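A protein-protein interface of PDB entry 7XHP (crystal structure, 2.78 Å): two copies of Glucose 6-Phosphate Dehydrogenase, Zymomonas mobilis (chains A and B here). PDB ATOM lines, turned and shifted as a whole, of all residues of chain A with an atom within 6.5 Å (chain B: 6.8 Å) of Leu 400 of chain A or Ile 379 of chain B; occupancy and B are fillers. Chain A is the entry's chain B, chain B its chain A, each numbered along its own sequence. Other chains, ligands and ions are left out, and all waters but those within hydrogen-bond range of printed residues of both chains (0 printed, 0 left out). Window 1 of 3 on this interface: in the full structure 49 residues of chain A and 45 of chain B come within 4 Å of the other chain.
O of Asp 401 of chain A is in hydrogen-bond range of N of Asp 401 of chain B (3.3 Å).
The backbone carbonyl oxygen (O) of Leu 402 of chain B lies within hydrogen-bond range of the backbone NH (N) of Ile 377 of chain B (2.9 Å). The backbone carbonyl oxygen (O) of Ile 379 of chain B is in hydrogen-bond range of the backbone NH (N) of Leu 400 of chain B. N of Ile 381 of chain B is in hydrogen-bond range of O of Val 398 of chain B, 2.7 Å away. The backbone carbonyl oxygen (O) of Ile 377 of chain A lies within hydrogen-bond range of the backbone NH (N) of Leu 402 of chain A, 2.9 Å away. O of Ile 379 of chain A lies within hydrogen-bond range of N of Leu 400 of chain A (2.7 Å). N of Ile 381 of chain A is in hydrogen-bond range of O of Val 398 of chain A (2.6 Å).
Among the printed residues, merely in contact across the chains: Leu 193 of chain A with Leu 193 of chain B, Leu 193 of chain A with Ile 379 of chain B, Ile 377 of chain A with Leu 400 of chain B, Gln 378 of chain A with Leu 400 of chain B, Ile 379 of chain A with Leu 193 of chain B, Ile 381 of chain A with Leu 402 of chain B, Val 398 of chain A with Leu 402 of chain B, Trp 399 of chain A with Leu 402 of chain B, Leu 400 of chain A with Ile 377 of chain B, Leu 400 of chain A with Gln 378 of chain B, Leu 400 of chain A with Ile 379 of chain B, Leu 400 of chain A with Leu 400 of chain B, Leu 400 of chain A with Asp 401 of chain B, Leu 400 of chain A with Leu 402 of chain B, Leu 402 of chain A with Val 398 of chain B, Leu 402 of chain A with Trp 399 of chain B and Leu 402 of chain A with Leu 400 of chain B.
Of the printed residues of chain B, Ile 377 of chain A touches Leu 400 (3.2 Å). Printed residues of chain B within 4 Å of Ile 381 of chain A: Leu 402. Of the printed residues of chain B, Trp 399 of chain A touches Leu 402 (3.5 Å). Leu 400 of chain A touches just these residues of chain B: Ile 377, Gln 378, Ile 379, Leu 400, Asp 401 and Leu 402. Lys 366 of chain B touches none of the printed residues of chain A. Of chain A, only Leu 193 and Leu 400 come within 4 Å of Ile 379 of chain B. Ile 381 of chain B touches none of the printed residues of chain A. The nearest residue of chain A that does not touch Ile 379 of chain B is Ile 379 of chain A (4.3 Å). The nearest printed residue of chain B that does not touch Trp 399 of chain A is Asp 401 of chain B (4.5 Å).
Of the 18 printed residues of chain B, 9 touch a printed residue of chain A. Printed residues of chain A that touch a printed residue of chain B: Leu 193, Ile 377, Gln 378, Ile 379, Ile 381, Val 398, Trp 399, Leu 400, Asp 401 and Leu 402. Hydrophobic or aromatic side chains of chain A that line the printed part of chain B: Leu 193, Ile 379, Ile 381, Val 398, Leu 400 and Leu 402. Among the printed residues, no Asp or Glu carboxylate lies within 4 Å of a Lys or Arg side-chain nitrogen of the other chain.
Gln 378 of chain A touches Leu 400 of chain B, and with the chains exchanged Leu 400 of chain A touches Gln 378 of chain B. Val 398 of chain A touches Leu 402 of chain B, and with the chains exchanged Leu 402 of chain A touches Val 398 of chain B. Leu 400 of chain A touches Asp 401 of chain B, but with the chains exchanged Asp 401 of chain A does not touch Leu 400 of chain B (4.1 Å). Leu 400 of chain A touches Leu 402 of chain B, and with the chains exchanged Leu 402 of chain A touches Leu 400 of chain B. 11 positions are printed for both chains.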
ATOM      1  N   LEU A 193     -12.214  30.715  36.182  1.00  0.00           N
ATOM      2  CA  LEU A 193     -13.490  30.238  35.680  1.00  0.00           C
ATOM      3  C   LEU A 193     -14.299  29.588  36.791  1.00  0.00           C
ATOM      4  O   LEU A 193     -15.518  29.426  36.652  1.00  0.00           O
ATOM      5  CB  LEU A 193     -13.244  29.264  34.523  1.00  0.00           C
ATOM      6  CG  LEU A 193     -14.342  28.326  34.025  1.00  0.00           C
ATOM      7  CD1 LEU A 193     -15.338  29.118  33.209  1.00  0.00           C
ATOM      8  CD2 LEU A 193     -13.751  27.205  33.193  1.00  0.00           C
ATOM      9  N   ILE A 377     -10.978  15.211  34.938  1.00  0.00           N
ATOM     10  CA  ILE A 377     -11.851  16.344  35.233  1.00  0.00           C
ATOM     11  C   ILE A 377     -12.793  16.550  34.052  1.00  0.00           C
ATOM     12  O   ILE A 377     -12.388  16.394  32.895  1.00  0.00           O
ATOM     13  CB  ILE A 377     -11.052  17.638  35.502  1.00  0.00           C
ATOM     14  CG1 ILE A 377      -9.838  17.358  36.391  1.00  0.00           C
ATOM     15  CG2 ILE A 377     -11.953  18.706  36.111  1.00  0.00           C
ATOM     16  CD1 ILE A 377      -9.271  18.586  37.063  1.00  0.00           C
ATOM     17  N   GLN A 378     -14.053  16.886  34.339  1.00  0.00           N
ATOM     18  CA  GLN A 378     -15.020  17.124  33.272  1.00  0.00           C
ATOM     19  C   GLN A 378     -16.014  18.196  33.701  1.00  0.00           C
ATOM     20  O   GLN A 378     -16.213  18.454  34.890  1.00  0.00           O
ATOM     21  CB  GLN A 378     -15.825  15.882  32.856  1.00  0.00           C
ATOM     22  CG  GLN A 378     -15.332  14.508  33.240  1.00  0.00           C
ATOM     23  CD  GLN A 378     -16.372  13.445  32.905  1.00  0.00           C
ATOM     24  OE1 GLN A 378     -16.895  12.762  33.786  1.00  0.00           O
ATOM     25  NE2 GLN A 378     -16.702  13.329  31.624  1.00  0.00           N
ATOM     26  N   ILE A 379     -16.639  18.817  32.699  1.00  0.00           N
ATOM     27  CA  ILE A 379     -17.628  19.874  32.881  1.00  0.00           C
ATOM     28  C   ILE A 379     -18.836  19.575  32.003  1.00  0.00           C
ATOM     29  O   ILE A 379     -18.702  19.011  30.915  1.00  0.00           O
ATOM     30  CB  ILE A 379     -17.007  21.249  32.546  1.00  0.00           C
ATOM     31  CG1 ILE A 379     -16.084  21.697  33.681  1.00  0.00           C
ATOM     32  CG2 ILE A 379     -18.072  22.294  32.241  1.00  0.00           C
ATOM     33  CD1 ILE A 379     -15.777  23.178  33.660  1.00  0.00           C
ATOM     34  N   SER A 380     -20.022  19.978  32.463  1.00  0.00           N
ATOM     35  CA  SER A 380     -21.285  19.644  31.810  1.00  0.00           C
ATOM     36  C   SER A 380     -21.833  20.870  31.097  1.00  0.00           C
ATOM     37  O   SER A 380     -22.115  21.887  31.739  1.00  0.00           O
ATOM     38  CB  SER A 380     -22.321  19.160  32.819  1.00  0.00           C
ATOM     39  OG  SER A 380     -21.748  18.288  33.753  1.00  0.00           O
ATOM     40  N   ILE A 381     -21.991  20.777  29.781  1.00  0.00           N
ATOM     41  CA  ILE A 381     -22.541  21.887  29.018  1.00  0.00           C
ATOM     42  C   ILE A 381     -23.743  21.405  28.223  1.00  0.00           C
ATOM     43  O   ILE A 381     -23.850  20.225  27.872  1.00  0.00           O
ATOM     44  CB  ILE A 381     -21.487  22.505  28.078  1.00  0.00           C
ATOM     45  CG1 ILE A 381     -20.976  21.451  27.097  1.00  0.00           C
ATOM     46  CG2 ILE A 381     -20.336  23.079  28.875  1.00  0.00           C
ATOM     47  CD1 ILE A 381     -20.265  22.025  25.900  1.00  0.00           C
ATOM     48  N   VAL A 398     -23.696  17.581  27.564  1.00  0.00           N
ATOM     49  CA  VAL A 398     -22.484  16.928  27.101  1.00  0.00           C
ATOM     50  C   VAL A 398     -21.349  17.414  27.982  1.00  0.00           C
ATOM     51  O   VAL A 398     -21.455  18.438  28.659  1.00  0.00           O
ATOM     52  CB  VAL A 398     -22.216  17.228  25.608  1.00  0.00           C
ATOM     53  CG1 VAL A 398     -23.100  16.363  24.723  1.00  0.00           C
ATOM     54  CG2 VAL A 398     -22.497  18.697  25.325  1.00  0.00           C
ATOM     55  N   TRP A 399     -20.253  16.669  27.976  1.00  0.00           N
ATOM     56  CA  TRP A 399     -19.215  16.823  28.983  1.00  0.00           C
ATOM     57  C   TRP A 399     -17.904  17.168  28.299  1.00  0.00           C
ATOM     58  O   TRP A 399     -17.448  16.435  27.414  1.00  0.00           O
ATOM     59  CB  TRP A 399     -19.048  15.546  29.811  1.00  0.00           C
ATOM     60  CG  TRP A 399     -20.107  15.290  30.855  1.00  0.00           C
ATOM     61  CD1 TRP A 399     -21.299  14.654  30.674  1.00  0.00           C
ATOM     62  CD2 TRP A 399     -20.044  15.632  32.249  1.00  0.00           C
ATOM     63  NE1 TRP A 399     -21.989  14.591  31.861  1.00  0.00           N
ATOM     64  CE2 TRP A 399     -21.240  15.183  32.843  1.00  0.00           C
ATOM     65  CE3 TRP A 399     -19.101  16.283  33.047  1.00  0.00           C
ATOM     66  CZ2 TRP A 399     -21.514  15.363  34.197  1.00  0.00           C
ATOM     67  CZ3 TRP A 399     -19.371  16.455  34.394  1.00  0.00           C
ATOM     68  CH2 TRP A 399     -20.564  15.991  34.957  1.00  0.00           C
ATOM     69  N   LEU A 400     -17.299  18.275  28.714  1.00  0.00           N
ATOM     70  CA  LEU A 400     -15.936  18.596  28.315  1.00  0.00           C
ATOM     71  C   LEU A 400     -14.995  17.792  29.199  1.00  0.00           C
ATOM     72  O   LEU A 400     -14.873  18.066  30.394  1.00  0.00           O
ATOM     73  CB  LEU A 400     -15.679  20.093  28.451  1.00  0.00           C
ATOM     74  CG  LEU A 400     -16.477  21.004  27.523  1.00  0.00           C
ATOM     75  CD1 LEU A 400     -16.913  22.234  28.276  1.00  0.00           C
ATOM     76  CD2 LEU A 400     -15.623  21.408  26.338  1.00  0.00           C
ATOM     77  N   ASP A 401     -14.326  16.807  28.612  1.00  0.00           N
ATOM     78  CA  ASP A 401     -13.583  15.805  29.360  1.00  0.00           C
ATOM     79  C   ASP A 401     -12.090  16.014  29.154  1.00  0.00           C
ATOM     80  O   ASP A 401     -11.635  16.284  28.039  1.00  0.00           O
ATOM     81  CB  ASP A 401     -13.988  14.381  28.954  1.00  0.00           C
ATOM     82  CG  ASP A 401     -14.325  14.263  27.483  1.00  0.00           C
ATOM     83  OD1 ASP A 401     -15.177  13.422  27.131  1.00  0.00           O
ATOM     84  OD2 ASP A 401     -13.738  15.007  26.677  1.00  0.00           O
ATOM     85  N   LEU A 402     -11.338  15.897  30.243  1.00  0.00           N
ATOM     86  CA  LEU A 402      -9.886  15.964  30.221  1.00  0.00           C
ATOM     87  C   LEU A 402      -9.332  14.800  31.026  1.00  0.00           C
ATOM     88  O   LEU A 402      -9.817  14.514  32.123  1.00  0.00           O
ATOM     89  CB  LEU A 402      -9.389  17.291  30.794  1.00  0.00           C
ATOM     90  CG  LEU A 402      -8.034  17.299  31.494  1.00  0.00           C
ATOM     91  CD1 LEU A 402      -6.899  17.106  30.501  1.00  0.00           C
ATOM     92  CD2 LEU A 402      -7.880  18.594  32.263  1.00  0.00           C
ATOM     93  N   LEU B 193     -22.969  28.629  33.241  1.00  0.00           N
ATOM     94  CA  LEU B 193     -21.559  28.879  33.514  1.00  0.00           C
ATOM     95  C   LEU B 193     -20.989  30.099  32.790  1.00  0.00           C
ATOM     96  O   LEU B 193     -19.971  30.640  33.237  1.00  0.00           O
ATOM     97  CB  LEU B 193     -20.748  27.644  33.106  1.00  0.00           C
ATOM     98  CG  LEU B 193     -19.601  27.072  33.942  1.00  0.00           C
ATOM     99  CD1 LEU B 193     -18.984  25.883  33.209  1.00  0.00           C
ATOM    100  CD2 LEU B 193     -18.554  28.114  34.256  1.00  0.00           C
ATOM    101  N   PHE B 194     -21.628  30.580  31.723  1.00  0.00           N
ATOM    102  CA  PHE B 194     -20.977  31.593  30.889  1.00  0.00           C
ATOM    103  C   PHE B 194     -21.352  33.034  31.225  1.00  0.00           C
ATOM    104  O   PHE B 194     -20.476  33.847  31.538  1.00  0.00           O
ATOM    105  CB  PHE B 194     -21.312  31.340  29.417  1.00  0.00           C
ATOM    106  CG  PHE B 194     -21.164  29.918  28.999  1.00  0.00           C
ATOM    107  CD1 PHE B 194     -19.912  29.388  28.743  1.00  0.00           C
ATOM    108  CD2 PHE B 194     -22.270  29.111  28.855  1.00  0.00           C
ATOM    109  CE1 PHE B 194     -19.770  28.075  28.353  1.00  0.00           C
ATOM    110  CE2 PHE B 194     -22.122  27.804  28.468  1.00  0.00           C
ATOM    111  CZ  PHE B 194     -20.889  27.283  28.216  1.00  0.00           C
ATOM    112  N   PHE B 347     -10.208  35.245  28.789  1.00  0.00           N
ATOM    113  CA  PHE B 347     -10.810  35.861  29.963  1.00  0.00           C
ATOM    114  C   PHE B 347      -9.774  36.638  30.775  1.00  0.00           C
ATOM    115  O   PHE B 347      -8.569  36.393  30.687  1.00  0.00           O
ATOM    116  CB  PHE B 347     -11.467  34.793  30.848  1.00  0.00           C
ATOM    117  CG  PHE B 347     -12.709  34.175  30.257  1.00  0.00           C
ATOM    118  CD1 PHE B 347     -12.615  33.083  29.405  1.00  0.00           C
ATOM    119  CD2 PHE B 347     -13.969  34.657  30.586  1.00  0.00           C
ATOM    120  CE1 PHE B 347     -13.746  32.505  28.870  1.00  0.00           C
ATOM    121  CE2 PHE B 347     -15.105  34.102  30.057  1.00  0.00           C
ATOM    122  CZ  PHE B 347     -14.999  33.014  29.197  1.00  0.00           C
ATOM    123  N   ASN B 365      -7.577  31.968  30.811  1.00  0.00           N
ATOM    124  CA  ASN B 365      -8.516  30.959  30.358  1.00  0.00           C
ATOM    125  C   ASN B 365      -8.976  31.289  28.948  1.00  0.00           C
ATOM    126  O   ASN B 365      -9.241  32.449  28.618  1.00  0.00           O
ATOM    127  CB  ASN B 365      -9.722  30.882  31.296  1.00  0.00           C
ATOM    128  CG  ASN B 365      -9.339  31.016  32.760  1.00  0.00           C
ATOM    129  OD1 ASN B 365      -9.081  32.116  33.252  1.00  0.00           O
ATOM    130  ND2 ASN B 365      -9.307  29.892  33.468  1.00  0.00           N
ATOM    131  N   LYS B 366      -9.060  30.270  28.107  1.00  0.00           N
ATOM    132  CA  LYS B 366      -9.598  30.444  26.771  1.00  0.00           C
ATOM    133  C   LYS B 366     -10.765  29.491  26.591  1.00  0.00           C
ATOM    134  O   LYS B 366     -10.699  28.320  26.981  1.00  0.00           O
ATOM    135  CB  LYS B 366      -8.544  30.204  25.679  1.00  0.00           C
ATOM    136  CG  LYS B 366      -7.175  30.787  25.986  1.00  0.00           C
ATOM    137  CD  LYS B 366      -6.084  29.773  25.712  1.00  0.00           C
ATOM    138  CE  LYS B 366      -4.977  29.853  26.744  1.00  0.00           C
ATOM    139  NZ  LYS B 366      -3.791  30.588  26.223  1.00  0.00           N
ATOM    140  N   LEU B 367     -11.822  30.008  25.990  1.00  0.00           N
ATOM    141  CA  LEU B 367     -12.969  29.220  25.578  1.00  0.00           C
ATOM    142  C   LEU B 367     -12.855  29.199  24.066  1.00  0.00           C
ATOM    143  O   LEU B 367     -13.002  30.235  23.408  1.00  0.00           O
ATOM    144  CB  LEU B 367     -14.273  29.851  26.062  1.00  0.00           C
ATOM    145  CG  LEU B 367     -15.623  29.352  25.539  1.00  0.00           C
ATOM    146  CD1 LEU B 367     -15.846  27.877  25.845  1.00  0.00           C
ATOM    147  CD2 LEU B 367     -16.755  30.203  26.115  1.00  0.00           C
ATOM    148  N   ARG B 368     -12.594  28.024  23.521  1.00  0.00           N
ATOM    149  CA  ARG B 368     -12.290  27.878  22.110  1.00  0.00           C
ATOM    150  C   ARG B 368     -13.435  27.143  21.445  1.00  0.00           C
ATOM    151  O   ARG B 368     -13.772  26.024  21.839  1.00  0.00           O
ATOM    152  CB  ARG B 368     -10.972  27.131  21.929  1.00  0.00           C
ATOM    153  CG  ARG B 368     -10.501  26.953  20.507  1.00  0.00           C
ATOM    154  CD  ARG B 368      -9.039  26.564  20.521  1.00  0.00           C
ATOM    155  NE  ARG B 368      -8.802  25.213  20.027  1.00  0.00           N
ATOM    156  CZ  ARG B 368      -8.760  24.880  18.745  1.00  0.00           C
ATOM    157  NH1 ARG B 368      -8.916  25.784  17.793  1.00  0.00           N
ATOM    158  NH2 ARG B 368      -8.553  23.611  18.411  1.00  0.00           N
ATOM    159  N   ILE B 377     -15.396  22.515  20.820  1.00  0.00           N
ATOM    160  CA  ILE B 377     -15.401  23.496  21.902  1.00  0.00           C
ATOM    161  C   ILE B 377     -14.465  22.997  23.000  1.00  0.00           C
ATOM    162  O   ILE B 377     -14.437  21.798  23.298  1.00  0.00           O
ATOM    163  CB  ILE B 377     -16.822  23.744  22.454  1.00  0.00           C
ATOM    164  CG1 ILE B 377     -17.808  24.013  21.315  1.00  0.00           C
ATOM    165  CG2 ILE B 377     -16.823  24.916  23.425  1.00  0.00           C
ATOM    166  CD1 ILE B 377     -19.236  23.684  21.659  1.00  0.00           C
ATOM    167  N   GLN B 378     -13.684  23.903  23.593  1.00  0.00           N
ATOM    168  CA  GLN B 378     -12.744  23.503  24.637  1.00  0.00           C
ATOM    169  C   GLN B 378     -12.479  24.653  25.603  1.00  0.00           C
ATOM    170  O   GLN B 378     -12.705  25.822  25.283  1.00  0.00           O
ATOM    171  CB  GLN B 378     -11.426  23.014  24.034  1.00  0.00           C
ATOM    172  CG  GLN B 378     -10.914  23.908  22.932  1.00  0.00           C
ATOM    173  CD  GLN B 378     -10.095  23.174  21.897  1.00  0.00           C
ATOM    174  OE1 GLN B 378     -10.359  23.271  20.701  1.00  0.00           O
ATOM    175  NE2 GLN B 378      -9.087  22.438  22.352  1.00  0.00           N
ATOM    176  N   ILE B 379     -11.998  24.302  26.804  1.00  0.00           N
ATOM    177  CA  ILE B 379     -11.637  25.270  27.837  1.00  0.00           C
ATOM    178  C   ILE B 379     -10.252  24.939  28.376  1.00  0.00           C
ATOM    179  O   ILE B 379      -9.880  23.770  28.502  1.00  0.00           O
ATOM    180  CB  ILE B 379     -12.643  25.300  29.009  1.00  0.00           C
ATOM    181  CG1 ILE B 379     -14.057  24.960  28.562  1.00  0.00           C
ATOM    182  CG2 ILE B 379     -12.644  26.646  29.693  1.00  0.00           C
ATOM    183  CD1 ILE B 379     -14.964  24.732  29.736  1.00  0.00           C
ATOM    184  N   SER B 380      -9.503  25.980  28.745  1.00  0.00           N
ATOM    185  CA  SER B 380      -8.111  25.858  29.167  1.00  0.00           C
ATOM    186  C   SER B 380      -7.991  26.143  30.658  1.00  0.00           C
ATOM    187  O   SER B 380      -8.280  27.260  31.098  1.00  0.00           O
ATOM    188  CB  SER B 380      -7.220  26.825  28.392  1.00  0.00           C
ATOM    189  OG  SER B 380      -7.690  26.995  27.074  1.00  0.00           O
ATOM    190  N   ILE B 381      -7.554  25.145  31.430  1.00  0.00           N
ATOM    191  CA  ILE B 381      -7.400  25.305  32.871  1.00  0.00           C
ATOM    192  C   ILE B 381      -6.007  24.887  33.325  1.00  0.00           C
ATOM    193  O   ILE B 381      -5.262  24.206  32.616  1.00  0.00           O
ATOM    194  CB  ILE B 381      -8.465  24.535  33.679  1.00  0.00           C
ATOM    195  CG1 ILE B 381      -8.273  23.027  33.534  1.00  0.00           C
ATOM    196  CG2 ILE B 381      -9.866  24.986  33.276  1.00  0.00           C
ATOM    197  CD1 ILE B 381      -9.399  22.225  34.120  1.00  0.00           C
ATOM    198  N   VAL B 398      -3.805  23.169  30.298  1.00  0.00           N
ATOM    199  CA  VAL B 398      -4.376  21.987  29.668  1.00  0.00           C
ATOM    200  C   VAL B 398      -5.830  22.293  29.334  1.00  0.00           C
ATOM    201  O   VAL B 398      -6.412  23.254  29.840  1.00  0.00           O
ATOM    202  CB  VAL B 398      -4.232  20.752  30.583  1.00  0.00           C
ATOM    203  CG1 VAL B 398      -5.226  20.825  31.718  1.00  0.00           C
ATOM    204  CG2 VAL B 398      -4.361  19.465  29.784  1.00  0.00           C
ATOM    205  N   TRP B 399      -6.422  21.473  28.465  1.00  0.00           N
ATOM    206  CA  TRP B 399      -7.688  21.799  27.818  1.00  0.00           C
ATOM    207  C   TRP B 399      -8.734  20.717  28.073  1.00  0.00           C
ATOM    208  O   TRP B 399      -8.495  19.540  27.783  1.00  0.00           O
ATOM    209  CB  TRP B 399      -7.492  21.963  26.306  1.00  0.00           C
ATOM    210  CG  TRP B 399      -6.686  23.158  25.883  1.00  0.00           C
ATOM    211  CD1 TRP B 399      -5.331  23.300  25.955  1.00  0.00           C
ATOM    212  CD2 TRP B 399      -7.185  24.362  25.288  1.00  0.00           C
ATOM    213  NE1 TRP B 399      -4.958  24.525  25.455  1.00  0.00           N
ATOM    214  CE2 TRP B 399      -6.078  25.195  25.037  1.00  0.00           C
ATOM    215  CE3 TRP B 399      -8.461  24.820  24.950  1.00  0.00           C
ATOM    216  CZ2 TRP B 399      -6.207  26.459  24.463  1.00  0.00           C
ATOM    217  CZ3 TRP B 399      -8.589  26.073  24.374  1.00  0.00           C
ATOM    218  CH2 TRP B 399      -7.469  26.877  24.138  1.00  0.00           C
ATOM    219  N   LEU B 400      -9.893  21.122  28.603  1.00  0.00           N
ATOM    220  CA  LEU B 400     -11.078  20.262  28.654  1.00  0.00           C
ATOM    221  C   LEU B 400     -11.772  20.327  27.297  1.00  0.00           C
ATOM    222  O   LEU B 400     -12.338  21.364  26.937  1.00  0.00           O
ATOM    223  CB  LEU B 400     -12.033  20.696  29.764  1.00  0.00           C
ATOM    224  CG  LEU B 400     -11.615  20.700  31.235  1.00  0.00           C
ATOM    225  CD1 LEU B 400     -12.209  21.913  31.935  1.00  0.00           C
ATOM    226  CD2 LEU B 400     -12.064  19.415  31.914  1.00  0.00           C
ATOM    227  N   ASP B 401     -11.747  19.227  26.551  1.00  0.00           N
ATOM    228  CA  ASP B 401     -12.103  19.223  25.136  1.00  0.00           C
ATOM    229  C   ASP B 401     -13.383  18.440  24.866  1.00  0.00           C
ATOM    230  O   ASP B 401     -13.564  17.338  25.393  1.00  0.00           O
ATOM    231  CB  ASP B 401     -10.953  18.640  24.311  1.00  0.00           C
ATOM    232  CG  ASP B 401     -10.812  19.303  22.960  1.00  0.00           C
ATOM    233  OD1 ASP B 401     -10.086  20.314  22.878  1.00  0.00           O
ATOM    234  OD2 ASP B 401     -11.426  18.819  21.984  1.00  0.00           O
ATOM    235  N   LEU B 402     -14.261  19.006  24.038  1.00  0.00           N
ATOM    236  CA  LEU B 402     -15.435  18.308  23.530  1.00  0.00           C
ATOM    237  C   LEU B 402     -15.567  18.588  22.038  1.00  0.00           C
ATOM    238  O   LEU B 402     -15.484  19.745  21.615  1.00  0.00           O
ATOM    239  CB  LEU B 402     -16.699  18.745  24.265  1.00  0.00           C
ATOM    240  CG  LEU B 402     -17.983  18.099  23.760  1.00  0.00           C
ATOM    241  CD1 LEU B 402     -17.954  16.591  23.950  1.00  0.00           C
ATOM    242  CD2 LEU B 402     -19.136  18.722  24.492  1.00  0.00           C
ATOM    243  N   SER B 403     -15.794  17.537  21.247  1.00  0.00           N
ATOM    244  CA  SER B 403     -15.926  17.651  19.797  1.00  0.00           C
ATOM    245  C   SER B 403     -17.295  17.159  19.338  1.00  0.00           C
ATOM    246  O   SER B 403     -17.626  15.981  19.504  1.00  0.00           O
ATOM    247  CB  SER B 403     -14.815  16.874  19.086  1.00  0.00           C
ATOM    248  OG  SER B 403     -15.337  15.757  18.392  1.00  0.00           O
